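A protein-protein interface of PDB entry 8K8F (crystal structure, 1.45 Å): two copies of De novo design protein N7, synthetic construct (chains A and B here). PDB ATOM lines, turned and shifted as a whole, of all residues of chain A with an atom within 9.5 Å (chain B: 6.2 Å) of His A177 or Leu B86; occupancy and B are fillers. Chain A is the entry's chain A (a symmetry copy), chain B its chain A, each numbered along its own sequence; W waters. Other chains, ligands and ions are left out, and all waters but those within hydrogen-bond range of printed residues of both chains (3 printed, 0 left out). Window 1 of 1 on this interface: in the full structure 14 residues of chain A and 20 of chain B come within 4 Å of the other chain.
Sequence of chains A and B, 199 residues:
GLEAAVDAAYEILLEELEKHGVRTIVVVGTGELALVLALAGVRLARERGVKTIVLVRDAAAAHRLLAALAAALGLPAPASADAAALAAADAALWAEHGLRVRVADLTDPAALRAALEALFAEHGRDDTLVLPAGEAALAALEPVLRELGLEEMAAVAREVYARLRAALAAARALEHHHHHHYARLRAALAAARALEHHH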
ATOM      1  N   GLY A   1      -6.482   7.742   9.217  1.00  0.00           N
ATOM      2  CA  GLY A   1      -7.887   8.088   9.116  1.00  0.00           C
ATOM      3  C   GLY A   1      -8.134   9.536   9.475  1.00  0.00           C
ATOM      4  O   GLY A   1      -7.202  10.264   9.812  1.00  0.00           O
ATOM      5  N   LEU A   2      -9.405   9.935   9.430  1.00  0.00           N
ATOM      6  CA  LEU A   2      -9.752  11.345   9.580  1.00  0.00           C
ATOM      7  C   LEU A   2      -9.478  11.854  10.991  1.00  0.00           C
ATOM      8  O   LEU A   2      -8.983  12.979  11.163  1.00  0.00           O
ATOM      9  CB  LEU A   2     -11.218  11.560   9.205  1.00  0.00           C
ATOM     10  CG  LEU A   2     -11.700  13.014   9.222  1.00  0.00           C
ATOM     11  CD1 LEU A   2     -10.881  13.876   8.262  1.00  0.00           C
ATOM     12  CD2 LEU A   2     -13.165  13.080   8.871  1.00  0.00           C
ATOM     13  N   GLU A   3      -9.796  11.058  12.016  1.00  0.00           N
ATOM     14  CA  GLU A   3      -9.590  11.520  13.385  1.00  0.00           C
ATOM     15  C   GLU A   3      -8.120  11.764  13.672  1.00  0.00           C
ATOM     16  O   GLU A   3      -7.761  12.767  14.305  1.00  0.00           O
ATOM     17  CB  GLU A   3     -10.190  10.538  14.393  1.00  0.00           C
ATOM     18  CG  GLU A   3     -11.664  10.303  14.138  1.00  0.00           C
ATOM     19  CD  GLU A   3     -11.976   9.003  13.432  1.00  0.00           C
ATOM     20  OE1 GLU A   3     -11.211   8.593  12.527  1.00  0.00           O
ATOM     21  OE2 GLU A   3     -13.053   8.437  13.740  1.00  0.00           O
ATOM     22  N   LEU A  35     -10.366  20.519   4.673  1.00  0.00           N
ATOM     23  CA  LEU A  35     -11.345  19.892   5.555  1.00  0.00           C
ATOM     24  C   LEU A  35     -10.749  19.631   6.930  1.00  0.00           C
ATOM     25  O   LEU A  35     -11.376  19.915   7.959  1.00  0.00           O
ATOM     26  CB  LEU A  35     -11.858  18.585   4.948  1.00  0.00           C
ATOM     27  CG  LEU A  35     -12.825  17.813   5.864  1.00  0.00           C
ATOM     28  CD1 LEU A  35     -14.036  18.671   6.229  1.00  0.00           C
ATOM     29  CD2 LEU A  35     -13.275  16.507   5.239  1.00  0.00           C
ATOM     30  N   ARG A  64     -19.200  21.761  -1.415  1.00  0.00           N
ATOM     31  CA  ARG A  64     -18.574  20.490  -1.069  1.00  0.00           C
ATOM     32  C   ARG A  64     -17.961  20.535   0.326  1.00  0.00           C
ATOM     33  O   ARG A  64     -18.097  19.584   1.101  1.00  0.00           O
ATOM     34  CB  ARG A  64     -17.544  20.097  -2.125  1.00  0.00           C
ATOM     35  CG  ARG A  64     -18.061  19.070  -3.125  1.00  0.00           C
ATOM     36  CD  ARG A  64     -16.991  18.651  -4.132  1.00  0.00           C
ATOM     37  NE  ARG A  64     -16.157  19.773  -4.541  1.00  0.00           N
ATOM     38  CZ  ARG A  64     -16.229  20.372  -5.724  1.00  0.00           C
ATOM     39  NH1 ARG A  64     -17.126  20.011  -6.629  1.00  0.00           N
ATOM     40  NH2 ARG A  64     -15.390  21.367  -5.999  1.00  0.00           N
ATOM     41  N   ALA A  67     -20.732  20.712   2.924  1.00  0.00           N
ATOM     42  CA  ALA A  67     -21.428  19.431   3.034  1.00  0.00           C
ATOM     43  C   ALA A  67     -20.635  18.444   3.879  1.00  0.00           C
ATOM     44  O   ALA A  67     -21.214  17.659   4.643  1.00  0.00           O
ATOM     45  CB  ALA A  67     -21.685  18.869   1.639  1.00  0.00           C
ATOM     46  N   ALA A  68     -19.308  18.454   3.743  1.00  0.00           N
ATOM     47  CA  ALA A  68     -18.474  17.584   4.567  1.00  0.00           C
ATOM     48  C   ALA A  68     -18.466  18.058   6.014  1.00  0.00           C
ATOM     49  O   ALA A  68     -18.526  17.246   6.942  1.00  0.00           O
ATOM     50  CB  ALA A  68     -17.055  17.544   4.005  1.00  0.00           C
ATOM     51  N   LEU A  69     -18.384  19.373   6.231  1.00  0.00           N
ATOM     52  CA  LEU A  69     -18.517  19.883   7.590  1.00  0.00           C
ATOM     53  C   LEU A  69     -19.868  19.501   8.189  1.00  0.00           C
ATOM     54  O   LEU A  69     -19.948  19.106   9.360  1.00  0.00           O
ATOM     55  CB  LEU A  69     -18.325  21.400   7.588  1.00  0.00           C
ATOM     56  CG  LEU A  69     -16.895  21.841   7.319  1.00  0.00           C
ATOM     57  CD1 LEU A  69     -16.873  23.345   7.103  1.00  0.00           C
ATOM     58  CD2 LEU A  69     -16.022  21.436   8.479  1.00  0.00           C
ATOM     59  N   ALA A  70     -20.946  19.618   7.402  1.00  0.00           N
ATOM     60  CA  ALA A  70     -22.270  19.250   7.896  1.00  0.00           C
ATOM     61  C   ALA A  70     -22.288  17.803   8.363  1.00  0.00           C
ATOM     62  O   ALA A  70     -22.745  17.499   9.471  1.00  0.00           O
ATOM     63  CB  ALA A  70     -23.311  19.478   6.799  1.00  0.00           C
ATOM     64  N   ALA A  71     -21.761  16.900   7.534  1.00  0.00           N
ATOM     65  CA  ALA A  71     -21.721  15.486   7.893  1.00  0.00           C
ATOM     66  C   ALA A  71     -20.939  15.263   9.180  1.00  0.00           C
ATOM     67  O   ALA A  71     -21.310  14.417  10.005  1.00  0.00           O
ATOM     68  CB  ALA A  71     -21.110  14.685   6.746  1.00  0.00           C
ATOM     69  N   ALA A  72     -19.843  16.005   9.367  1.00  0.00           N
ATOM     70  CA  ALA A  72     -19.051  15.835  10.579  1.00  0.00           C
ATOM     71  C   ALA A  72     -19.805  16.319  11.808  1.00  0.00           C
ATOM     72  O   ALA A  72     -19.586  15.802  12.910  1.00  0.00           O
ATOM     73  CB  ALA A  72     -17.713  16.567  10.443  1.00  0.00           C
ATOM     74  N   ARG A 172      -3.237  10.205   6.857  1.00  0.00           N
ATOM     75  CA  ARG A 172      -4.065   9.626   5.792  1.00  0.00           C
ATOM     76  C   ARG A 172      -5.560   9.777   6.097  1.00  0.00           C
ATOM     77  O   ARG A 172      -6.270   8.813   6.392  1.00  0.00           O
ATOM     78  CB  ARG A 172      -3.683   8.163   5.533  1.00  0.00           C
ATOM     79  CG  ARG A 172      -2.175   7.923   5.552  1.00  0.00           C
ATOM     80  CD  ARG A 172      -1.886   6.492   5.992  1.00  0.00           C
ATOM     81  NE  ARG A 172      -2.576   6.193   7.246  1.00  0.00           N
ATOM     82  CZ  ARG A 172      -2.516   5.038   7.896  1.00  0.00           C
ATOM     83  NH1 ARG A 172      -1.776   4.033   7.455  1.00  0.00           N
ATOM     84  NH2 ARG A 172      -3.217   4.888   9.017  1.00  0.00           N
ATOM     85  N   ALA A 173      -6.026  11.025   5.984  1.00  0.00           N
ATOM     86  CA  ALA A 173      -7.387  11.358   6.405  1.00  0.00           C
ATOM     87  C   ALA A 173      -8.441  10.544   5.662  1.00  0.00           C
ATOM     88  O   ALA A 173      -9.456  10.156   6.248  1.00  0.00           O
ATOM     89  CB  ALA A 173      -7.655  12.851   6.210  1.00  0.00           C
ATOM     90  N   LEU A 174      -8.239  10.295   4.369  1.00  0.00           N
ATOM     91  CA  LEU A 174      -9.280   9.709   3.532  1.00  0.00           C
ATOM     92  C   LEU A 174      -9.022   8.248   3.179  1.00  0.00           C
ATOM     93  O   LEU A 174      -9.729   7.702   2.322  1.00  0.00           O
ATOM     94  CB  LEU A 174      -9.460  10.534   2.256  1.00  0.00           C
ATOM     95  CG  LEU A 174      -9.809  11.998   2.501  1.00  0.00           C
ATOM     96  CD1 LEU A 174     -10.069  12.716   1.184  1.00  0.00           C
ATOM     97  CD2 LEU A 174     -11.010  12.108   3.430  1.00  0.00           C
ATOM     98  N   GLU A 175      -8.046   7.604   3.829  1.00  0.00           N
ATOM     99  CA  GLU A 175      -7.610   6.265   3.428  1.00  0.00           C
ATOM    100  C   GLU A 175      -8.736   5.237   3.471  1.00  0.00           C
ATOM    101  O   GLU A 175      -8.702   4.257   2.719  1.00  0.00           O
ATOM    102  CB  GLU A 175      -6.456   5.807   4.316  1.00  0.00           C
ATOM    103  CG  GLU A 175      -6.806   5.702   5.790  1.00  0.00           C
ATOM    104  CD  GLU A 175      -5.682   5.119   6.624  1.00  0.00           C
ATOM    105  OE1 GLU A 175      -4.868   4.324   6.092  1.00  0.00           O
ATOM    106  OE2 GLU A 175      -5.610   5.451   7.825  1.00  0.00           O
ATOM    107  N   HIS A 176      -9.715   5.421   4.345  1.00  0.00           N
ATOM    108  CA  HIS A 176     -10.751   4.416   4.538  1.00  0.00           C
ATOM    109  C   HIS A 176     -11.964   4.668   3.656  1.00  0.00           C
ATOM    110  O   HIS A 176     -12.979   3.966   3.787  1.00  0.00           O
ATOM    111  CB  HIS A 176     -11.161   4.386   6.009  1.00  0.00           C
ATOM    112  CG  HIS A 176     -10.058   3.985   6.932  1.00  0.00           C
ATOM    113  ND1 HIS A 176      -9.320   2.830   6.760  1.00  0.00           N
ATOM    114  CD2 HIS A 176      -9.512   4.624   7.996  1.00  0.00           C
ATOM    115  CE1 HIS A 176      -8.397   2.758   7.703  1.00  0.00           C
ATOM    116  NE2 HIS A 176      -8.490   3.836   8.464  1.00  0.00           N
ATOM    117  N   HIS A 177     -11.897   5.657   2.759  1.00  0.00           N
ATOM    118  CA  HIS A 177     -13.097   6.037   2.023  1.00  0.00           C
ATOM    119  C   HIS A 177     -12.865   6.207   0.524  1.00  0.00           C
ATOM    120  O   HIS A 177     -13.656   6.881  -0.150  1.00  0.00           O
ATOM    121  CB  HIS A 177     -13.779   7.214   2.720  1.00  0.00           C
ATOM    122  CG  HIS A 177     -14.281   6.847   4.080  1.00  0.00           C
ATOM    123  ND1 HIS A 177     -13.544   7.050   5.228  1.00  0.00           N
ATOM    124  CD2 HIS A 177     -15.406   6.198   4.465  1.00  0.00           C
ATOM    125  CE1 HIS A 177     -14.205   6.563   6.264  1.00  0.00           C
ATOM    126  NE2 HIS A 177     -15.343   6.055   5.831  1.00  0.00           N
ATOM    127  N   HIS A 178     -11.810   5.591  -0.003  1.00  0.00           N
ATOM    128  CA  HIS A 178     -11.591   5.452  -1.436  1.00  0.00           C
ATOM    129  C   HIS A 178     -10.684   4.250  -1.666  1.00  0.00           C
ATOM    130  O   HIS A 178     -10.073   3.725  -0.733  1.00  0.00           O
ATOM    131  CB  HIS A 178     -11.036   6.738  -2.064  1.00  0.00           C
ATOM    132  CG  HIS A 178      -9.579   6.962  -1.815  1.00  0.00           C
ATOM    133  ND1 HIS A 178      -9.101   7.472  -0.628  1.00  0.00           N
ATOM    134  CD2 HIS A 178      -8.497   6.760  -2.603  1.00  0.00           C
ATOM    135  CE1 HIS A 178      -7.785   7.572  -0.693  1.00  0.00           C
ATOM    136  NE2 HIS A 178      -7.393   7.143  -1.880  1.00  0.00           N
ATOM    137  N   HIS A 179     -10.643   3.790  -2.912  1.00  0.00           N
ATOM    138  CA  HIS A 179      -9.757   2.688  -3.256  1.00  0.00           C
ATOM    139  C   HIS A 179      -8.318   3.161  -3.388  1.00  0.00           C
ATOM    140  O   HIS A 179      -8.059   4.249  -3.915  1.00  0.00           O
ATOM    141  CB  HIS A 179     -10.204   2.017  -4.554  1.00  0.00           C
ATOM    142  CG  HIS A 179     -11.484   1.248  -4.431  1.00  0.00           C
ATOM    143  ND1 HIS A 179     -12.107   0.653  -5.510  1.00  0.00           N
ATOM    144  CD2 HIS A 179     -12.255   0.968  -3.354  1.00  0.00           C
ATOM    145  CE1 HIS A 179     -13.212   0.051  -5.103  1.00  0.00           C
ATOM    146  NE2 HIS A 179     -13.327   0.231  -3.801  1.00  0.00           N
ATOM    147  N   ASP B  58     -17.436   0.033  -2.415  1.00  0.00           N
ATOM    148  CA  ASP B  58     -17.042   1.292  -3.037  1.00  0.00           C
ATOM    149  C   ASP B  58     -17.743   2.459  -2.352  1.00  0.00           C
ATOM    150  O   ASP B  58     -18.577   2.271  -1.462  1.00  0.00           O
ATOM    151  CB  ASP B  58     -17.229   1.260  -4.561  1.00  0.00           C
ATOM    152  CG  ASP B  58     -18.676   1.073  -4.984  1.00  0.00           C
ATOM    153  OD1 ASP B  58     -19.585   1.049  -4.121  1.00  0.00           O
ATOM    154  OD2 ASP B  58     -18.906   0.954  -6.205  1.00  0.00           O
ATOM    155  N   ALA B  59     -17.367   3.680  -2.765  1.00  0.00           N
ATOM    156  CA  ALA B  59     -17.918   4.884  -2.147  1.00  0.00           C
ATOM    157  C   ALA B  59     -19.429   4.976  -2.337  1.00  0.00           C
ATOM    158  O   ALA B  59     -20.152   5.403  -1.428  1.00  0.00           O
ATOM    159  CB  ALA B  59     -17.226   6.127  -2.712  1.00  0.00           C
ATOM    160  N   ALA B  60     -19.927   4.575  -3.510  1.00  0.00           N
ATOM    161  CA  ALA B  60     -21.370   4.562  -3.733  1.00  0.00           C
ATOM    162  C   ALA B  60     -22.074   3.654  -2.731  1.00  0.00           C
ATOM    163  O   ALA B  60     -23.104   4.025  -2.163  1.00  0.00           O
ATOM    164  CB  ALA B  60     -21.677   4.136  -5.168  1.00  0.00           C
ATOM    165  N   ALA B  62     -20.975   2.915   0.244  1.00  0.00           N
ATOM    166  CA  ALA B  62     -20.880   3.543   1.559  1.00  0.00           C
ATOM    167  C   ALA B  62     -21.944   4.612   1.724  1.00  0.00           C
ATOM    168  O   ALA B  62     -22.579   4.711   2.784  1.00  0.00           O
ATOM    169  CB  ALA B  62     -19.485   4.136   1.769  1.00  0.00           C
ATOM    170  N   HIS B  63     -22.163   5.408   0.681  1.00  0.00           N
ATOM    171  CA  HIS B  63     -23.220   6.406   0.747  1.00  0.00           C
ATOM    172  C   HIS B  63     -24.588   5.765   0.944  1.00  0.00           C
ATOM    173  O   HIS B  63     -25.392   6.243   1.754  1.00  0.00           O
ATOM    174  CB  HIS B  63     -23.220   7.267  -0.505  1.00  0.00           C
ATOM    175  CG  HIS B  63     -24.222   8.376  -0.446  1.00  0.00           C
ATOM    176  ND1 HIS B  63     -25.538   8.214  -0.828  1.00  0.00           N
ATOM    177  CD2 HIS B  63     -24.124   9.633   0.044  1.00  0.00           C
ATOM    178  CE1 HIS B  63     -26.192   9.344  -0.623  1.00  0.00           C
ATOM    179  NE2 HIS B  63     -25.356  10.220  -0.098  1.00  0.00           N
ATOM    180  N   LEU B  66     -24.729   4.513   4.565  1.00  0.00           N
ATOM    181  CA  LEU B  66     -24.808   5.644   5.485  1.00  0.00           C
ATOM    182  C   LEU B  66     -26.154   6.354   5.387  1.00  0.00           C
ATOM    183  O   LEU B  66     -26.674   6.838   6.397  1.00  0.00           O
ATOM    184  CB  LEU B  66     -23.665   6.632   5.231  1.00  0.00           C
ATOM    185  CG  LEU B  66     -22.302   6.121   5.684  1.00  0.00           C
ATOM    186  CD1 LEU B  66     -21.187   6.898   4.993  1.00  0.00           C
ATOM    187  CD2 LEU B  66     -22.173   6.236   7.196  1.00  0.00           C
ATOM    188  N   PRO B  78     -25.308  11.883   4.217  1.00  0.00           N
ATOM    189  CA  PRO B  78     -24.229  12.680   3.615  1.00  0.00           C
ATOM    190  C   PRO B  78     -24.679  13.181   2.254  1.00  0.00           C
ATOM    191  O   PRO B  78     -25.366  12.480   1.512  1.00  0.00           O
ATOM    192  CB  PRO B  78     -23.078  11.676   3.467  1.00  0.00           C
ATOM    193  CG  PRO B  78     -23.447  10.525   4.367  1.00  0.00           C
ATOM    194  CD  PRO B  78     -24.930  10.469   4.390  1.00  0.00           C
ATOM    195  N   SER B  80     -23.254  13.558  -0.539  1.00  0.00           N
ATOM    196  CA  SER B  80     -22.802  12.834  -1.721  1.00  0.00           C
ATOM    197  C   SER B  80     -21.838  11.742  -1.284  1.00  0.00           C
ATOM    198  O   SER B  80     -21.547  11.585  -0.097  1.00  0.00           O
ATOM    199  CB  SER B  80     -22.134  13.774  -2.727  1.00  0.00           C
ATOM    200  OG  SER B  80     -20.797  14.056  -2.341  1.00  0.00           O
ATOM    201  N   ALA B  81     -21.349  10.982  -2.263  1.00  0.00           N
ATOM    202  CA  ALA B  81     -20.341   9.957  -2.033  1.00  0.00           C
ATOM    203  C   ALA B  81     -18.921  10.499  -2.124  1.00  0.00           C
ATOM    204  O   ALA B  81     -17.979   9.715  -2.254  1.00  0.00           O
ATOM    205  CB  ALA B  81     -20.517   8.788  -3.008  1.00  0.00           C
ATOM    206  N   ASP B  82     -18.761  11.820  -2.111  1.00  0.00           N
ATOM    207  CA  ASP B  82     -17.452  12.435  -1.938  1.00  0.00           C
ATOM    208  C   ASP B  82     -16.718  11.804  -0.760  1.00  0.00           C
ATOM    209  O   ASP B  82     -17.289  11.633   0.320  1.00  0.00           O
ATOM    210  CB  ASP B  82     -17.690  13.924  -1.690  1.00  0.00           C
ATOM    211  CG  ASP B  82     -16.419  14.714  -1.580  1.00  0.00           C
ATOM    212  OD1 ASP B  82     -15.561  14.622  -2.484  1.00  0.00           O
ATOM    213  OD2 ASP B  82     -16.312  15.455  -0.585  1.00  0.00           O
ATOM    214  N   ALA B  83     -15.442  11.458  -0.971  1.00  0.00           N
ATOM    215  CA  ALA B  83     -14.683  10.775   0.076  1.00  0.00           C
ATOM    216  C   ALA B  83     -14.626  11.600   1.355  1.00  0.00           C
ATOM    217  O   ALA B  83     -14.728  11.058   2.460  1.00  0.00           O
ATOM    218  CB  ALA B  83     -13.279  10.417  -0.416  1.00  0.00           C
ATOM    219  N   ALA B  84     -14.446  12.914   1.232  1.00  0.00           N
ATOM    220  CA  ALA B  84     -14.426  13.751   2.426  1.00  0.00           C
ATOM    221  C   ALA B  84     -15.764  13.722   3.154  1.00  0.00           C
ATOM    222  O   ALA B  84     -15.806  13.705   4.391  1.00  0.00           O
ATOM    223  CB  ALA B  84     -14.059  15.181   2.044  1.00  0.00           C
ATOM    224  N   ALA B  85     -16.872  13.756   2.410  1.00  0.00           N
ATOM    225  CA  ALA B  85     -18.187  13.679   3.039  1.00  0.00           C
ATOM    226  C   ALA B  85     -18.393  12.331   3.720  1.00  0.00           C
ATOM    227  O   ALA B  85     -18.926  12.268   4.835  1.00  0.00           O
ATOM    228  CB  ALA B  85     -19.285  13.923   2.002  1.00  0.00           C
ATOM    229  N   LEU B  86     -17.970  11.245   3.068  1.00  0.00           N
ATOM    230  CA  LEU B  86     -18.096   9.917   3.667  1.00  0.00           C
ATOM    231  C   LEU B  86     -17.215   9.781   4.905  1.00  0.00           C
ATOM    232  O   LEU B  86     -17.649   9.229   5.924  1.00  0.00           O
ATOM    233  CB  LEU B  86     -17.728   8.856   2.634  1.00  0.00           C
ATOM    234  CG  LEU B  86     -18.604   8.788   1.381  1.00  0.00           C
ATOM    235  CD1 LEU B  86     -18.030   7.750   0.440  1.00  0.00           C
ATOM    236  CD2 LEU B  86     -20.067   8.464   1.716  1.00  0.00           C
ATOM    237  N   ALA B  87     -15.980  10.291   4.848  1.00  0.00           N
ATOM    238  CA  ALA B  87     -15.106  10.182   6.009  1.00  0.00           C
ATOM    239  C   ALA B  87     -15.645  10.997   7.175  1.00  0.00           C
ATOM    240  O   ALA B  87     -15.549  10.576   8.336  1.00  0.00           O
ATOM    241  CB  ALA B  87     -13.670  10.594   5.654  1.00  0.00           C
ATOM    242  N   ALA B  88     -16.179  12.188   6.893  1.00  0.00           N
ATOM    243  CA  ALA B  88     -16.753  12.991   7.962  1.00  0.00           C
ATOM    244  C   ALA B  88     -17.976  12.317   8.564  1.00  0.00           C
ATOM    245  O   ALA B  88     -18.127  12.275   9.789  1.00  0.00           O
ATOM    246  CB  ALA B  88     -17.089  14.383   7.433  1.00  0.00           C
ATOM    247  N   ALA B  89     -18.861  11.797   7.717  1.00  0.00           N
ATOM    248  CA  ALA B  89     -20.027  11.075   8.217  1.00  0.00           C
ATOM    249  C   ALA B  89     -19.605   9.867   9.050  1.00  0.00           C
ATOM    250  O   ALA B  89     -20.201   9.587  10.100  1.00  0.00           O
ATOM    251  CB  ALA B  89     -20.900  10.643   7.042  1.00  0.00           C
ATOM    252  N   ASP B  90     -18.575   9.148   8.599  1.00  0.00           N
ATOM    253  CA  ASP B  90     -18.090   7.992   9.344  1.00  0.00           C
ATOM    254  C   ASP B  90     -17.561   8.392  10.712  1.00  0.00           C
ATOM    255  O   ASP B  90     -17.839   7.722  11.714  1.00  0.00           O
ATOM    256  CB  ASP B  90     -17.034   7.255   8.522  1.00  0.00           C
ATOM    257  CG  ASP B  90     -16.290   6.206   9.327  1.00  0.00           C
ATOM    258  OD1 ASP B  90     -16.808   5.066   9.348  1.00  0.00           O
ATOM    259  OD2 ASP B  90     -15.176   6.469   9.861  1.00  0.00           O
ATOM    260  N   ALA B  91     -16.786   9.479  10.782  1.00  0.00           N
ATOM    261  CA  ALA B  91     -16.258   9.898  12.073  1.00  0.00           C
ATOM    262  C   ALA B  91     -17.376  10.290  13.028  1.00  0.00           C
ATOM    263  O   ALA B  91     -17.299  10.013  14.231  1.00  0.00           O
ATOM    264  CB  ALA B  91     -15.296  11.071  11.887  1.00  0.00           C
ATOM    265  N   VAL B 101     -18.512   2.971   8.702  1.00  0.00           N
ATOM    266  CA  VAL B 101     -18.708   2.475   7.345  1.00  0.00           C
ATOM    267  C   VAL B 101     -17.475   2.882   6.555  1.00  0.00           C
ATOM    268  O   VAL B 101     -17.233   4.081   6.350  1.00  0.00           O
ATOM    269  CB  VAL B 101     -19.976   3.033   6.690  1.00  0.00           C
ATOM    270  CG1 VAL B 101     -20.090   2.496   5.278  1.00  0.00           C
ATOM    271  CG2 VAL B 101     -21.200   2.681   7.513  1.00  0.00           C
ATOM    272  N   ARG B 102     -16.688   1.893   6.127  1.00  0.00           N
ATOM    273  CA  ARG B 102     -15.454   2.104   5.383  1.00  0.00           C
ATOM    274  C   ARG B 102     -15.546   1.436   4.020  1.00  0.00           C
ATOM    275  O   ARG B 102     -16.326   0.500   3.809  1.00  0.00           O
ATOM    276  CB  ARG B 102     -14.235   1.547   6.126  1.00  0.00           C
ATOM    277  CG  ARG B 102     -13.976   2.187   7.468  1.00  0.00           C
ATOM    278  CD  ARG B 102     -12.671   1.657   8.041  1.00  0.00           C
ATOM    279  NE  ARG B 102     -12.181   2.500   9.120  1.00  0.00           N
ATOM    280  CZ  ARG B 102     -11.242   2.154   9.987  1.00  0.00           C
ATOM    281  NH1 ARG B 102     -10.682   0.951   9.961  1.00  0.00           N
ATOM    282  NH2 ARG B 102     -10.858   3.035  10.908  1.00  0.00           N
ATOM    283  N   VAL B 103     -14.734   1.933   3.096  1.00  0.00           N
ATOM    284  CA  VAL B 103     -14.640   1.415   1.737  1.00  0.00           C
ATOM    285  C   VAL B 103     -13.459   0.457   1.652  1.00  0.00           C
ATOM    286  O   VAL B 103     -12.326   0.815   2.009  1.00  0.00           O
ATOM    287  CB  VAL B 103     -14.467   2.567   0.730  1.00  0.00           C
ATOM    288  CG1 VAL B 103     -14.202   2.010  -0.659  1.00  0.00           C
ATOM    289  CG2 VAL B 103     -15.694   3.466   0.723  1.00  0.00           C
HETATM  290  O   HOH W   1     -18.482  16.917   0.548  1.00  0.00           O
HETATM  291  O   HOH W   2     -14.799   9.858  15.438  1.00  0.00           O
HETATM  292  O   HOH W   3     -10.648   6.416  11.287  1.00  0.00           O
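N of Val B103 lies within hydrogen-bond range of O of His A176 (2.8 Å).
The guanidinium group of Arg B102 sits at hydrogen-bond distance from a ring nitrogen (NE2) of His A176, 3.5 Å away.
The backbone carbonyl oxygen (O) of Val B101 is in hydrogen-bond range of a ring nitrogen (NE2) of His A177 (2.8 Å).
A ring nitrogen (NE2) of His A176 sits at hydrogen-bond distance from the side-chain carboxylate (OE2) of Glu A175 (3.4 Å).
O of Leu A174 lies within hydrogen-bond range of ND1 of His A178 (3.0 Å).
The backbone carbonyl oxygen (O) of Ala A173 lies within hydrogen-bond range of the backbone NH (N) of Leu A2, 3.2 Å away.
The side-chain carboxylate (OD2) of Asp B82 lies within hydrogen-bond range of the backbone NH (N) of Ala B85 (3.5 Å).
The side-chain carboxylate (OD1) of Asp B90 sits at hydrogen-bond distance from the backbone NH (N) of Val B101, at 2.8 Å.
Leu A2 touches Ala B87 (CD2 to O, 3.5 Å).
Leu A35 touches Ala B84.
CB of Ala B88 touches O of Ala A68, at 3.2 Å.
Ala B85 touches Ala A71 (O to CB, 3.8 Å).
O of Ala B88 touches O of Ala A71, at 3.8 Å.
Leu B86 touches His A177.
His A177 touches Ala B87 (ND1 to CB, 3.6 Å).
Asp B90 touches His A177.
His A177 touches Arg B102 (NE2 to CA, 3.98 Å).
CD2 of His A179 touches CG1 of Val B103, at 3.5 Å.
Of the printed residues of chain B, Ala A68 touches Ala B88.
Of the printed residues of chain B, Leu A174 touches Ala B83 (3.98 Å), Ala B84 (3.9 Å) and Ala B87 (3.8 Å).
His A177 touches seven residues of chain B.
Printed residues of chain A within 4 Å of Asp B58: His A179.
Ala B59 touches none of the printed residues of chain A.
No residue of chain A comes within 4 Å of Ala B81.
Of chain A, only Ala A71 (3.8 Å) comes within 4 Å of Ala B85.
Leu B86 touches just one residue of chain A: His A177.
Ala B87 touches just these residues of chain A: Leu A2 (3.5 Å), Leu A174 (3.8 Å) and His A177 (3.6 Å).
Ala B89 touches just one residue of chain A: Ala A71 (3.8 Å).
Printed residues of chain A within 4 Å of Val B103: His A176 (2.8 Å), His A177 (3.9 Å) and His A179 (3.5 Å).
The nearest residue of chain B that does not touch His A177 is Ala B59 (4.5 Å).
The nearest residue of chain A that does not touch Leu B86 is Ala A71 (5.9 Å).
Of the 19 printed residues of chain A, 10 touch a printed residue of chain B.
Hydrophobic or aromatic side chains of chain A that line the printed part of chain B: Leu A2, Leu A35, Ala A71, Ala A72, Leu A174, His A176, His A177 and His A179.
Along chain A the printed residues that touch a printed residue of chain B span positions 2 to 179.
Of the 22 printed residues of chain B, 13 touch a printed residue of chain A.
Printed residues of chain B that touch a printed residue of chain A: Asp B58, Ala B83, Ala B84, Ala B85, Leu B86, Ala B87, Ala B88, Ala B89, Asp B90, Ala B91, Val B101, Arg B102 and Val B103.
Hydrophobic or aromatic side chains of chain B within 4 Å of the printed part of chain A: Ala B83, Ala B84, Leu B86, Ala B87, Ala B88, Ala B91 and Val B103.
Among the printed residues, 23 pairs touch across the chains.
No position is printed for both chains.
Of the 23 pairs that touch across the chains among the printed residues, none has its exchanged pair printed and touching as well.
Water W3 lies within hydrogen-bond range of the side-chain carboxylate (OE1) of Glu A3 (2.6 Å) and the guanidinium group (NH2) of Arg B102 (3.4 Å).
Water W1 lies within hydrogen-bond range of O of Arg A64 (2.8 Å) and OD2 of Asp B82 (2.9 Å).
Water W2 lies within hydrogen-bond range of O of Ala B91 (2.8 Å) and OE2 of Glu A3 (2.8 Å).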
